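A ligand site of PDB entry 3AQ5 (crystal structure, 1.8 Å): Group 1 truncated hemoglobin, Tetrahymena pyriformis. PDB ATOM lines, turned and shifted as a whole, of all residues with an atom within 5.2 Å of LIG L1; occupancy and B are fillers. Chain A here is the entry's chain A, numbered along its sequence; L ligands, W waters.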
ATOM      1  N   VAL A  34     -26.956  13.321  -9.659  1.00  0.00           N
ATOM      2  CA  VAL A  34     -27.203  13.826  -8.330  1.00  0.00           C
ATOM      3  C   VAL A  34     -28.351  14.863  -8.125  1.00  0.00           C
ATOM      4  O   VAL A  34     -28.704  15.141  -6.977  1.00  0.00           O
ATOM      5  CB  VAL A  34     -25.896  14.456  -7.671  1.00  0.00           C
ATOM      6  CG1 VAL A  34     -24.907  13.301  -7.290  1.00  0.00           C
ATOM      7  CG2 VAL A  34     -25.282  15.466  -8.569  1.00  0.00           C
ATOM      8  N   PHE A  37     -31.384  14.445  -5.570  1.00  0.00           N
ATOM      9  CA  PHE A  37     -31.252  14.428  -4.121  1.00  0.00           C
ATOM     10  C   PHE A  37     -31.743  15.737  -3.481  1.00  0.00           C
ATOM     11  O   PHE A  37     -32.141  15.738  -2.328  1.00  0.00           O
ATOM     12  CB  PHE A  37     -29.825  14.141  -3.665  1.00  0.00           C
ATOM     13  CG  PHE A  37     -29.455  12.717  -3.875  1.00  0.00           C
ATOM     14  CD1 PHE A  37     -28.746  12.391  -4.985  1.00  0.00           C
ATOM     15  CD2 PHE A  37     -29.879  11.739  -3.018  1.00  0.00           C
ATOM     16  CE1 PHE A  37     -28.424  11.080  -5.304  1.00  0.00           C
ATOM     17  CE2 PHE A  37     -29.595  10.359  -3.329  1.00  0.00           C
ATOM     18  CZ  PHE A  37     -28.857  10.051  -4.462  1.00  0.00           C
ATOM     19  N   PHE A  38     -31.708  16.801  -4.289  1.00  0.00           N
ATOM     20  CA  PHE A  38     -32.068  18.120  -3.839  1.00  0.00           C
ATOM     21  C   PHE A  38     -33.487  18.516  -4.119  1.00  0.00           C
ATOM     22  O   PHE A  38     -33.834  19.689  -3.925  1.00  0.00           O
ATOM     23  CB  PHE A  38     -31.113  19.139  -4.474  1.00  0.00           C
ATOM     24  CG  PHE A  38     -29.671  18.901  -4.097  1.00  0.00           C
ATOM     25  CD1 PHE A  38     -28.850  18.051  -4.864  1.00  0.00           C
ATOM     26  CD2 PHE A  38     -29.208  19.418  -2.897  1.00  0.00           C
ATOM     27  CE1 PHE A  38     -27.537  17.730  -4.441  1.00  0.00           C
ATOM     28  CE2 PHE A  38     -27.854  19.145  -2.454  1.00  0.00           C
ATOM     29  CZ  PHE A  38     -27.056  18.303  -3.216  1.00  0.00           C
ATOM     30  N   ASN A  40     -36.324  18.246  -2.590  1.00  0.00           N
ATOM     31  CA  ASN A  40     -37.118  18.881  -1.480  1.00  0.00           C
ATOM     32  C   ASN A  40     -36.291  19.849  -0.623  1.00  0.00           C
ATOM     33  O   ASN A  40     -36.748  20.307   0.419  1.00  0.00           O
ATOM     34  CB  ASN A  40     -37.668  17.805  -0.561  1.00  0.00           C
ATOM     35  CG  ASN A  40     -38.696  16.982  -1.269  1.00  0.00           C
ATOM     36  OD1 ASN A  40     -39.516  17.509  -1.977  1.00  0.00           O
ATOM     37  ND2 ASN A  40     -38.604  15.674  -1.139  1.00  0.00           N
ATOM     38  N   THR A  41     -35.158  20.285  -1.143  1.00  0.00           N
ATOM     39  CA  THR A  41     -34.206  21.070  -0.379  1.00  0.00           C
ATOM     40  C   THR A  41     -34.392  22.569  -0.650  1.00  0.00           C
ATOM     41  O   THR A  41     -34.654  22.983  -1.804  1.00  0.00           O
ATOM     42  CB  THR A  41     -32.752  20.662  -0.740  1.00  0.00           C
ATOM     43  OG1 THR A  41     -32.483  19.311  -0.286  1.00  0.00           O
ATOM     44  CG2 THR A  41     -31.699  21.549   0.044  1.00  0.00           C
ATOM     45  N   ASP A  42     -34.380  23.361   0.442  1.00  0.00           N
ATOM     46  CA  ASP A  42     -34.462  24.805   0.352  1.00  0.00           C
ATOM     47  C   ASP A  42     -33.072  25.236  -0.166  1.00  0.00           C
ATOM     48  O   ASP A  42     -32.059  25.185   0.616  1.00  0.00           O
ATOM     49  CB  ASP A  42     -34.721  25.349   1.762  1.00  0.00           C
ATOM     50  CG  ASP A  42     -34.651  26.849   1.863  1.00  0.00           C
ATOM     51  OD1 ASP A  42     -34.075  27.595   0.976  1.00  0.00           O
ATOM     52  OD2 ASP A  42     -35.302  27.316   2.856  1.00  0.00           O
ATOM     53  N   HIS A  45     -31.176  28.074   1.725  1.00  0.00           N
ATOM     54  CA  HIS A  45     -30.546  27.549   2.920  1.00  0.00           C
ATOM     55  C   HIS A  45     -29.333  26.757   2.639  1.00  0.00           C
ATOM     56  O   HIS A  45     -28.245  26.855   3.347  1.00  0.00           O
ATOM     57  CB  HIS A  45     -31.526  26.658   3.710  1.00  0.00           C
ATOM     58  CG  HIS A  45     -31.059  26.418   5.117  1.00  0.00           C
ATOM     59  ND1 HIS A  45     -30.622  25.192   5.560  1.00  0.00           N
ATOM     60  CD2 HIS A  45     -30.848  27.308   6.137  1.00  0.00           C
ATOM     61  CE1 HIS A  45     -30.252  25.307   6.833  1.00  0.00           C
ATOM     62  NE2 HIS A  45     -30.380  26.562   7.196  1.00  0.00           N
ATOM     63  N   GLN A  46     -29.474  25.800   1.726  1.00  0.00           N
ATOM     64  CA  GLN A  46     -28.363  24.930   1.374  1.00  0.00           C
ATOM     65  C   GLN A  46     -27.141  25.726   0.848  1.00  0.00           C
ATOM     66  O   GLN A  46     -25.976  25.410   1.154  1.00  0.00           O
ATOM     67  CB  GLN A  46     -28.861  23.906   0.312  1.00  0.00           C
ATOM     68  CG  GLN A  46     -27.729  22.977  -0.208  1.00  0.00           C
ATOM     69  CD  GLN A  46     -27.300  21.970   0.893  1.00  0.00           C
ATOM     70  OE1 GLN A  46     -27.988  21.902   1.980  1.00  0.00           O
ATOM     71  NE2 GLN A  46     -26.151  21.315   0.696  1.00  0.00           N
ATOM     72  N   GLN A  49     -25.446  27.212   3.966  1.00  0.00           N
ATOM     73  CA  GLN A  49     -24.686  26.219   4.731  1.00  0.00           C
ATOM     74  C   GLN A  49     -23.451  25.776   4.003  1.00  0.00           C
ATOM     75  O   GLN A  49     -22.373  25.608   4.610  1.00  0.00           O
ATOM     76  CB  GLN A  49     -25.543  24.957   5.036  1.00  0.00           C
ATOM     77  CG  GLN A  49     -26.749  25.365   5.917  1.00  0.00           C
ATOM     78  CD  GLN A  49     -26.244  25.994   7.254  1.00  0.00           C
ATOM     79  OE1 GLN A  49     -25.438  25.396   7.921  1.00  0.00           O
ATOM     80  NE2 GLN A  49     -26.656  27.099   7.591  1.00  0.00           N
ATOM     81  N   GLN A  50     -23.568  25.487   2.715  1.00  0.00           N
ATOM     82  CA  GLN A  50     -22.410  24.979   1.968  1.00  0.00           C
ATOM     83  C   GLN A  50     -21.340  26.069   1.791  1.00  0.00           C
ATOM     84  O   GLN A  50     -20.141  25.781   1.922  1.00  0.00           O
ATOM     85  CB  GLN A  50     -22.891  24.504   0.539  1.00  0.00           C
ATOM     86  CG  GLN A  50     -21.717  23.896  -0.310  1.00  0.00           C
ATOM     87  CD  GLN A  50     -21.309  22.487   0.267  1.00  0.00           C
ATOM     88  OE1 GLN A  50     -20.491  22.396   1.219  1.00  0.00           O
ATOM     89  NE2 GLN A  50     -22.114  21.481  -0.084  1.00  0.00           N
ATOM     90  N   PHE A  53     -19.693  26.024   5.098  1.00  0.00           N
ATOM     91  CA  PHE A  53     -18.939  24.804   5.333  1.00  0.00           C
ATOM     92  C   PHE A  53     -17.647  24.797   4.527  1.00  0.00           C
ATOM     93  O   PHE A  53     -16.550  24.547   5.079  1.00  0.00           O
ATOM     94  CB  PHE A  53     -19.759  23.544   4.918  1.00  0.00           C
ATOM     95  CG  PHE A  53     -19.077  22.281   5.340  1.00  0.00           C
ATOM     96  CD1 PHE A  53     -18.954  21.988   6.691  1.00  0.00           C
ATOM     97  CD2 PHE A  53     -18.647  21.342   4.385  1.00  0.00           C
ATOM     98  CE1 PHE A  53     -18.377  20.778   7.135  1.00  0.00           C
ATOM     99  CE2 PHE A  53     -18.036  20.117   4.828  1.00  0.00           C
ATOM    100  CZ  PHE A  53     -17.886  19.836   6.199  1.00  0.00           C
ATOM    101  N   LEU A  54     -17.713  25.096   3.224  1.00  0.00           N
ATOM    102  CA  LEU A  54     -16.474  25.095   2.431  1.00  0.00           C
ATOM    103  C   LEU A  54     -15.555  26.217   2.863  1.00  0.00           C
ATOM    104  O   LEU A  54     -14.329  26.101   2.767  1.00  0.00           O
ATOM    105  CB  LEU A  54     -16.772  25.231   0.921  1.00  0.00           C
ATOM    106  CG  LEU A  54     -17.521  23.961   0.380  1.00  0.00           C
ATOM    107  CD1 LEU A  54     -17.946  24.271  -1.152  1.00  0.00           C
ATOM    108  CD2 LEU A  54     -16.841  22.605   0.610  1.00  0.00           C
ATOM    109  N   LEU A  57     -13.790  24.830   5.750  1.00  0.00           N
ATOM    110  CA  LEU A  57     -12.896  23.655   5.476  1.00  0.00           C
ATOM    111  C   LEU A  57     -11.607  24.122   4.784  1.00  0.00           C
ATOM    112  O   LEU A  57     -10.499  23.516   4.980  1.00  0.00           O
ATOM    113  CB  LEU A  57     -13.581  22.731   4.463  1.00  0.00           C
ATOM    114  CG  LEU A  57     -13.627  21.231   4.673  1.00  0.00           C
ATOM    115  CD1 LEU A  57     -13.844  20.796   6.254  1.00  0.00           C
ATOM    116  CD2 LEU A  57     -14.687  20.584   3.870  1.00  0.00           C
ATOM    117  N   TYR A  64     -19.375  27.955  10.468  1.00  0.00           N
ATOM    118  CA  TYR A  64     -20.231  26.823  10.036  1.00  0.00           C
ATOM    119  C   TYR A  64     -20.928  26.276  11.266  1.00  0.00           C
ATOM    120  O   TYR A  64     -20.251  25.833  12.215  1.00  0.00           O
ATOM    121  CB  TYR A  64     -19.408  25.723   9.441  1.00  0.00           C
ATOM    122  CG  TYR A  64     -20.322  24.570   9.042  1.00  0.00           C
ATOM    123  CD1 TYR A  64     -21.343  24.794   8.114  1.00  0.00           C
ATOM    124  CD2 TYR A  64     -20.217  23.319   9.676  1.00  0.00           C
ATOM    125  CE1 TYR A  64     -22.198  23.738   7.742  1.00  0.00           C
ATOM    126  CE2 TYR A  64     -21.052  22.258   9.340  1.00  0.00           C
ATOM    127  CZ  TYR A  64     -22.072  22.488   8.368  1.00  0.00           C
ATOM    128  OH  TYR A  64     -22.926  21.417   8.044  1.00  0.00           O
ATOM    129  N   GLY A  66     -23.700  24.152  10.948  1.00  0.00           N
ATOM    130  CA  GLY A  66     -24.557  23.027  10.504  1.00  0.00           C
ATOM    131  C   GLY A  66     -24.200  21.627  11.018  1.00  0.00           C
ATOM    132  O   GLY A  66     -23.380  21.430  11.974  1.00  0.00           O
ATOM    133  N   LYS A  67     -24.862  20.635  10.424  1.00  0.00           N
ATOM    134  CA  LYS A  67     -24.737  19.307  10.810  1.00  0.00           C
ATOM    135  C   LYS A  67     -23.332  18.758  10.385  1.00  0.00           C
ATOM    136  O   LYS A  67     -22.747  19.270   9.473  1.00  0.00           O
ATOM    137  CB  LYS A  67     -25.781  18.468  10.063  1.00  0.00           C
ATOM    138  CG  LYS A  67     -27.258  18.771  10.681  1.00  0.00           C
ATOM    139  CD  LYS A  67     -28.243  18.049   9.721  1.00  0.00           C
ATOM    140  CE  LYS A  67     -29.741  18.447  10.165  1.00  0.00           C
ATOM    141  NZ  LYS A  67     -30.627  17.339   9.637  1.00  0.00           N
ATOM    142  N   MET A  69     -20.992  15.682   8.633  1.00  0.00           N
ATOM    143  CA  MET A  69     -21.245  15.119   7.315  1.00  0.00           C
ATOM    144  C   MET A  69     -21.998  13.805   7.396  1.00  0.00           C
ATOM    145  O   MET A  69     -22.589  13.412   6.393  1.00  0.00           O
ATOM    146  CB  MET A  69     -19.911  15.002   6.541  1.00  0.00           C
ATOM    147  CG  MET A  69     -19.370  16.420   6.175  1.00  0.00           C
ATOM    148  SD  MET A  69     -20.518  17.349   5.054  1.00  0.00           S
ATOM    149  CE  MET A  69     -21.360  18.455   6.178  1.00  0.00           C
ATOM    150  N   ALA A  72     -25.701  15.130   8.174  1.00  0.00           N
ATOM    151  CA  ALA A  72     -26.218  15.857   6.945  1.00  0.00           C
ATOM    152  C   ALA A  72     -26.798  14.887   5.865  1.00  0.00           C
ATOM    153  O   ALA A  72     -27.806  15.218   5.254  1.00  0.00           O
ATOM    154  CB  ALA A  72     -25.211  16.717   6.349  1.00  0.00           C
ATOM    155  N   HIS A  73     -26.206  13.704   5.727  1.00  0.00           N
ATOM    156  CA  HIS A  73     -26.542  12.796   4.634  1.00  0.00           C
ATOM    157  C   HIS A  73     -27.166  11.488   5.165  1.00  0.00           C
ATOM    158  O   HIS A  73     -27.199  10.458   4.439  1.00  0.00           O
ATOM    159  CB  HIS A  73     -25.285  12.525   3.776  1.00  0.00           C
ATOM    160  CG  HIS A  73     -24.680  13.821   3.278  1.00  0.00           C
ATOM    161  ND1 HIS A  73     -23.632  14.471   3.920  1.00  0.00           N
ATOM    162  CD2 HIS A  73     -25.122  14.656   2.331  1.00  0.00           C
ATOM    163  CE1 HIS A  73     -23.368  15.618   3.283  1.00  0.00           C
ATOM    164  NE2 HIS A  73     -24.252  15.740   2.301  1.00  0.00           N
ATOM    165  N   MET A  76     -29.621   8.719   3.308  1.00  0.00           N
ATOM    166  CA  MET A  76     -29.524   8.862   1.877  1.00  0.00           C
ATOM    167  C   MET A  76     -28.797   7.644   1.246  1.00  0.00           C
ATOM    168  O   MET A  76     -28.987   7.381   0.067  1.00  0.00           O
ATOM    169  CB  MET A  76     -28.791  10.112   1.454  1.00  0.00           C
ATOM    170  CG  MET A  76     -29.532  11.427   1.944  1.00  0.00           C
ATOM    171  SD  MET A  76     -28.501  12.809   1.374  1.00  0.00           S
ATOM    172  CE  MET A  76     -29.189  14.274   2.213  1.00  0.00           C
ATOM    173  N   LEU A  78     -25.779   7.233   0.335  1.00  0.00           N
ATOM    174  CA  LEU A  78     -25.052   7.760  -0.788  1.00  0.00           C
ATOM    175  C   LEU A  78     -23.979   6.744  -1.222  1.00  0.00           C
ATOM    176  O   LEU A  78     -23.374   6.035  -0.371  1.00  0.00           O
ATOM    177  CB  LEU A  78     -24.334   9.084  -0.440  1.00  0.00           C
ATOM    178  CG  LEU A  78     -25.340  10.224  -0.232  1.00  0.00           C
ATOM    179  CD1 LEU A  78     -24.539  11.476   0.172  1.00  0.00           C
ATOM    180  CD2 LEU A  78     -26.251  10.574  -1.434  1.00  0.00           C
ATOM    181  N   HIS A  82     -21.946   9.146  -6.435  1.00  0.00           N
ATOM    182  CA  HIS A  82     -22.561  10.438  -6.103  1.00  0.00           C
ATOM    183  C   HIS A  82     -21.482  11.409  -5.578  1.00  0.00           C
ATOM    184  O   HIS A  82     -21.458  12.564  -5.950  1.00  0.00           O
ATOM    185  CB  HIS A  82     -23.568  10.283  -5.003  1.00  0.00           C
ATOM    186  CG  HIS A  82     -24.689   9.318  -5.344  1.00  0.00           C
ATOM    187  ND1 HIS A  82     -25.534   9.477  -6.450  1.00  0.00           N
ATOM    188  CD2 HIS A  82     -25.143   8.236  -4.667  1.00  0.00           C
ATOM    189  CE1 HIS A  82     -26.414   8.457  -6.476  1.00  0.00           C
ATOM    190  NE2 HIS A  82     -26.214   7.721  -5.400  1.00  0.00           N
ATOM    191  N   PHE A  83     -20.555  10.878  -4.759  1.00  0.00           N
ATOM    192  CA  PHE A  83     -19.520  11.771  -4.245  1.00  0.00           C
ATOM    193  C   PHE A  83     -18.576  12.191  -5.390  1.00  0.00           C
ATOM    194  O   PHE A  83     -18.217  13.375  -5.443  1.00  0.00           O
ATOM    195  CB  PHE A  83     -18.741  10.998  -3.159  1.00  0.00           C
ATOM    196  CG  PHE A  83     -17.766  11.917  -2.396  1.00  0.00           C
ATOM    197  CD1 PHE A  83     -18.147  12.465  -1.205  1.00  0.00           C
ATOM    198  CD2 PHE A  83     -16.455  12.083  -2.886  1.00  0.00           C
ATOM    199  CE1 PHE A  83     -17.306  13.291  -0.447  1.00  0.00           C
ATOM    200  CE2 PHE A  83     -15.592  12.922  -2.194  1.00  0.00           C
ATOM    201  CZ  PHE A  83     -15.984  13.517  -0.988  1.00  0.00           C
ATOM    202  N   ILE A  86     -20.205  15.049  -7.168  1.00  0.00           N
ATOM    203  CA  ILE A  86     -20.044  16.345  -6.432  1.00  0.00           C
ATOM    204  C   ILE A  86     -18.644  16.940  -6.623  1.00  0.00           C
ATOM    205  O   ILE A  86     -18.526  18.120  -6.949  1.00  0.00           O
ATOM    206  CB  ILE A  86     -20.391  16.207  -4.917  1.00  0.00           C
ATOM    207  CG1 ILE A  86     -21.833  15.787  -4.813  1.00  0.00           C
ATOM    208  CG2 ILE A  86     -19.894  17.484  -4.079  1.00  0.00           C
ATOM    209  CD1 ILE A  86     -22.848  16.828  -5.403  1.00  0.00           C
ATOM    210  N   ILE A 111     -11.374  18.244   0.730  1.00  0.00           N
ATOM    211  CA  ILE A 111     -12.827  17.804   0.722  1.00  0.00           C
ATOM    212  C   ILE A 111     -12.924  16.288   0.623  1.00  0.00           C
ATOM    213  O   ILE A 111     -13.827  15.666   1.193  1.00  0.00           O
ATOM    214  CB  ILE A 111     -13.547  18.456  -0.432  1.00  0.00           C
ATOM    215  CG1 ILE A 111     -13.526  19.953  -0.166  1.00  0.00           C
ATOM    216  CG2 ILE A 111     -15.040  17.921  -0.647  1.00  0.00           C
ATOM    217  CD1 ILE A 111     -13.827  20.877  -1.414  1.00  0.00           C
ATOM    218  N   THR A 114     -13.864  13.854   3.470  1.00  0.00           N
ATOM    219  CA  THR A 114     -15.251  13.696   4.023  1.00  0.00           C
ATOM    220  C   THR A 114     -15.963  12.500   3.429  1.00  0.00           C
ATOM    221  O   THR A 114     -17.059  12.148   3.893  1.00  0.00           O
ATOM    222  CB  THR A 114     -16.123  14.944   3.774  1.00  0.00           C
ATOM    223  OG1 THR A 114     -16.351  15.168   2.349  1.00  0.00           O
ATOM    224  CG2 THR A 114     -15.498  16.192   4.435  1.00  0.00           C
ATOM    225  N   MET A 118     -19.843  10.362   4.799  1.00  0.00           N
ATOM    226  CA  MET A 118     -21.230  10.526   4.251  1.00  0.00           C
ATOM    227  C   MET A 118     -21.676   9.341   3.432  1.00  0.00           C
ATOM    228  O   MET A 118     -22.838   9.253   3.115  1.00  0.00           O
ATOM    229  CB  MET A 118     -21.369  11.865   3.519  1.00  0.00           C
ATOM    230  CG  MET A 118     -20.367  11.938   2.256  1.00  0.00           C
ATOM    231  SD  MET A 118     -20.645  13.487   1.403  1.00  0.00           S
ATOM    232  CE  MET A 118     -19.832  14.644   2.544  1.00  0.00           C
ATOM    233  N   LEU A 119     -20.747   8.494   2.943  1.00  0.00           N
ATOM    234  CA  LEU A 119     -21.269   7.380   2.121  1.00  0.00           C
ATOM    235  C   LEU A 119     -22.000   6.303   2.985  1.00  0.00           C
ATOM    236  O   LEU A 119     -21.552   5.948   4.057  1.00  0.00           O
ATOM    237  CB  LEU A 119     -20.161   6.631   1.334  1.00  0.00           C
ATOM    238  CG  LEU A 119     -19.447   7.578   0.332  1.00  0.00           C
ATOM    239  CD1 LEU A 119     -18.527   6.660  -0.495  1.00  0.00           C
ATOM    240  CD2 LEU A 119     -20.505   8.263  -0.556  1.00  0.00           C
HETATM  241  C1  LIG L   1     -26.703  18.653   3.105  1.00  0.00           C
HETATM  242  C2  LIG L   1     -26.770  15.976  -0.945  1.00  0.00           C
HETATM  243  C3  LIG L   1     -21.957  15.562  -0.760  1.00  0.00           C
HETATM  244  C4  LIG L   1     -21.958  19.292   2.336  1.00  0.00           C
HETATM  245  C5  LIG L   1     -27.153  17.999   1.996  1.00  0.00           C
HETATM  246  C6  LIG L   1     -28.572  17.803   1.547  1.00  0.00           C
HETATM  247  C7  LIG L   1     -28.541  17.109   0.405  1.00  0.00           C
HETATM  248  C8  LIG L   1     -27.153  16.763   0.100  1.00  0.00           C
HETATM  249  C9  LIG L   1     -29.726  16.644  -0.487  1.00  0.00           C
HETATM  250  C10 LIG L   1     -29.757  18.559   2.216  1.00  0.00           C
HETATM  251  C11 LIG L   1     -30.679  17.576   2.843  1.00  0.00           C
HETATM  252  C12 LIG L   1     -31.863  18.545   3.237  1.00  0.00           C
HETATM  253  O1  LIG L   1     -31.953  18.609   4.491  1.00  0.00           O
HETATM  254  O2  LIG L   1     -32.524  19.309   2.446  1.00  0.00           O
HETATM  255  C13 LIG L   1     -25.481  15.541  -1.179  1.00  0.00           C
HETATM  256  C14 LIG L   1     -25.117  14.535  -2.162  1.00  0.00           C
HETATM  257  C15 LIG L   1     -23.802  14.378  -2.030  1.00  0.00           C
HETATM  258  C16 LIG L   1     -23.293  15.325  -1.068  1.00  0.00           C
HETATM  259  C17 LIG L   1     -25.976  13.757  -3.162  1.00  0.00           C
HETATM  260  C18 LIG L   1     -22.958  13.392  -2.886  1.00  0.00           C
HETATM  261  C19 LIG L   1     -22.169  12.663  -2.155  1.00  0.00           C
HETATM  262  C20 LIG L   1     -21.525  16.633  -0.009  1.00  0.00           C
HETATM  263  C21 LIG L   1     -20.144  17.082   0.147  1.00  0.00           C
HETATM  264  C22 LIG L   1     -20.184  18.135   1.005  1.00  0.00           C
HETATM  265  C23 LIG L   1     -21.560  18.348   1.442  1.00  0.00           C
HETATM  266  C24 LIG L   1     -18.941  16.426  -0.671  1.00  0.00           C
HETATM  267  C25 LIG L   1     -19.040  19.041   1.528  1.00  0.00           C
HETATM  268  C26 LIG L   1     -17.774  18.617   1.309  1.00  0.00           C
HETATM  269  C27 LIG L   1     -23.209  19.427   2.848  1.00  0.00           C
HETATM  270  C28 LIG L   1     -23.569  20.416   3.815  1.00  0.00           C
HETATM  271  C29 LIG L   1     -25.006  20.222   4.087  1.00  0.00           C
HETATM  272  C30 LIG L   1     -25.421  19.151   3.211  1.00  0.00           C
HETATM  273  C31 LIG L   1     -22.698  21.512   4.495  1.00  0.00           C
HETATM  274  C32 LIG L   1     -25.839  21.086   5.018  1.00  0.00           C
HETATM  275  C33 LIG L   1     -25.936  20.434   6.358  1.00  0.00           C
HETATM  276  C34 LIG L   1     -26.816  21.348   7.212  1.00  0.00           C
HETATM  277  O3  LIG L   1     -26.662  21.427   8.439  1.00  0.00           O
HETATM  278  O4  LIG L   1     -27.839  21.921   6.676  1.00  0.00           O
HETATM  279  N1  LIG L   1     -26.427  17.303   1.080  1.00  0.00           N
HETATM  280  N2  LIG L   1     -24.363  16.045  -0.500  1.00  0.00           N
HETATM  281  N3  LIG L   1     -22.275  17.373   0.805  1.00  0.00           N
HETATM  282  N4  LIG L   1     -24.324  18.691   2.451  1.00  0.00           N
HETATM  283 FE1  LIG L   1     -24.337  17.314   0.973  1.00  0.00          FE
HETATM  284  O1  LG2 L   2     -24.411  18.925  -0.525  1.00  0.00           O
HETATM  285  O2  LG2 L   2     -23.916  19.314  -1.757  1.00  0.00           O
HETATM  286  O   HOH W   1     -29.189  22.671   4.080  1.00  0.00           O
HETATM  287  O   HOH W   2     -29.372  17.253   6.128  1.00  0.00           O
HETATM  288  O   HOH W   3     -28.346  22.593  10.161  1.00  0.00           O
HETATM  289  O   HOH W   4     -33.724  22.238   2.942  1.00  0.00           O
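NE2 of His 73 binds FE1 of LIG L1.
The side-chain hydroxyl (OG1) of Thr 41 sits at hydrogen-bond distance from an oxygen (O2) of LIG L1 (2.7 Å).
The backbone NH (N) of Lys 67 lies within hydrogen-bond range of an oxygen (O3) of LIG L1 (2.8 Å).
O2 of LG2 L2 sits at hydrogen-bond distance from NE2 of Gln 50 (3.3 Å).
The side-chain amide nitrogen of Gln 46 lies close to an oxygen (O1) of LG2 L2, 3.2 Å away.
An oxygen (O1) of LG2 L2 binds an iron atom (FE1) of LIG L1, 2.2 Å away.
The backbone carbonyl oxygen of Met 69 is in hydrogen-bond range of a ring nitrogen (ND1) of His 73 (2.9 Å).
O of Lys 67 sits at hydrogen-bond distance from OH of Tyr 64 (2.6 Å).
The backbone carbonyl oxygen (O) of Ile 111 sits at hydrogen-bond distance from the side-chain hydroxyl (OG1) of Thr 114 (2.8 Å).
Merely in contact with LIG L1: Phe 37, Phe 38, Gln 50, Met 118, Ile 86, Gly 66, Gln 46, Met 76, Ile 111, Phe 83, His 82, Leu 78, Tyr 64, Phe 53, Met 69, Gln 49, Ala 72 and Thr 114.
Hydrophobic or aromatic side chains within 4 Å of LIG L1: Phe 37, Phe 38, Phe 53, Tyr 64, Met 69, Ala 72, His 73, Met 76, Leu 78, His 82, Phe 83, Ile 86, Ile 111 and Met 118.
The nearest printed residue that does not touch LIG L1 is Leu 54 (4.2 Å).
Water W1 lies within hydrogen-bond range of the side-chain amide oxygen (OE1) of Gln 46 (2.5 Å), an oxygen (O4) of LIG L1 (3.0 Å) and a ring nitrogen (ND1) of His 45 (3.3 Å).
Water W4 bridges the backbone NH of Asp 42 and an oxygen (O2) of LIG L1.
Water W2 lies within hydrogen-bond range of O of Ala 72 (2.7 Å) and O1 of LIG L1 (3.3 Å).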
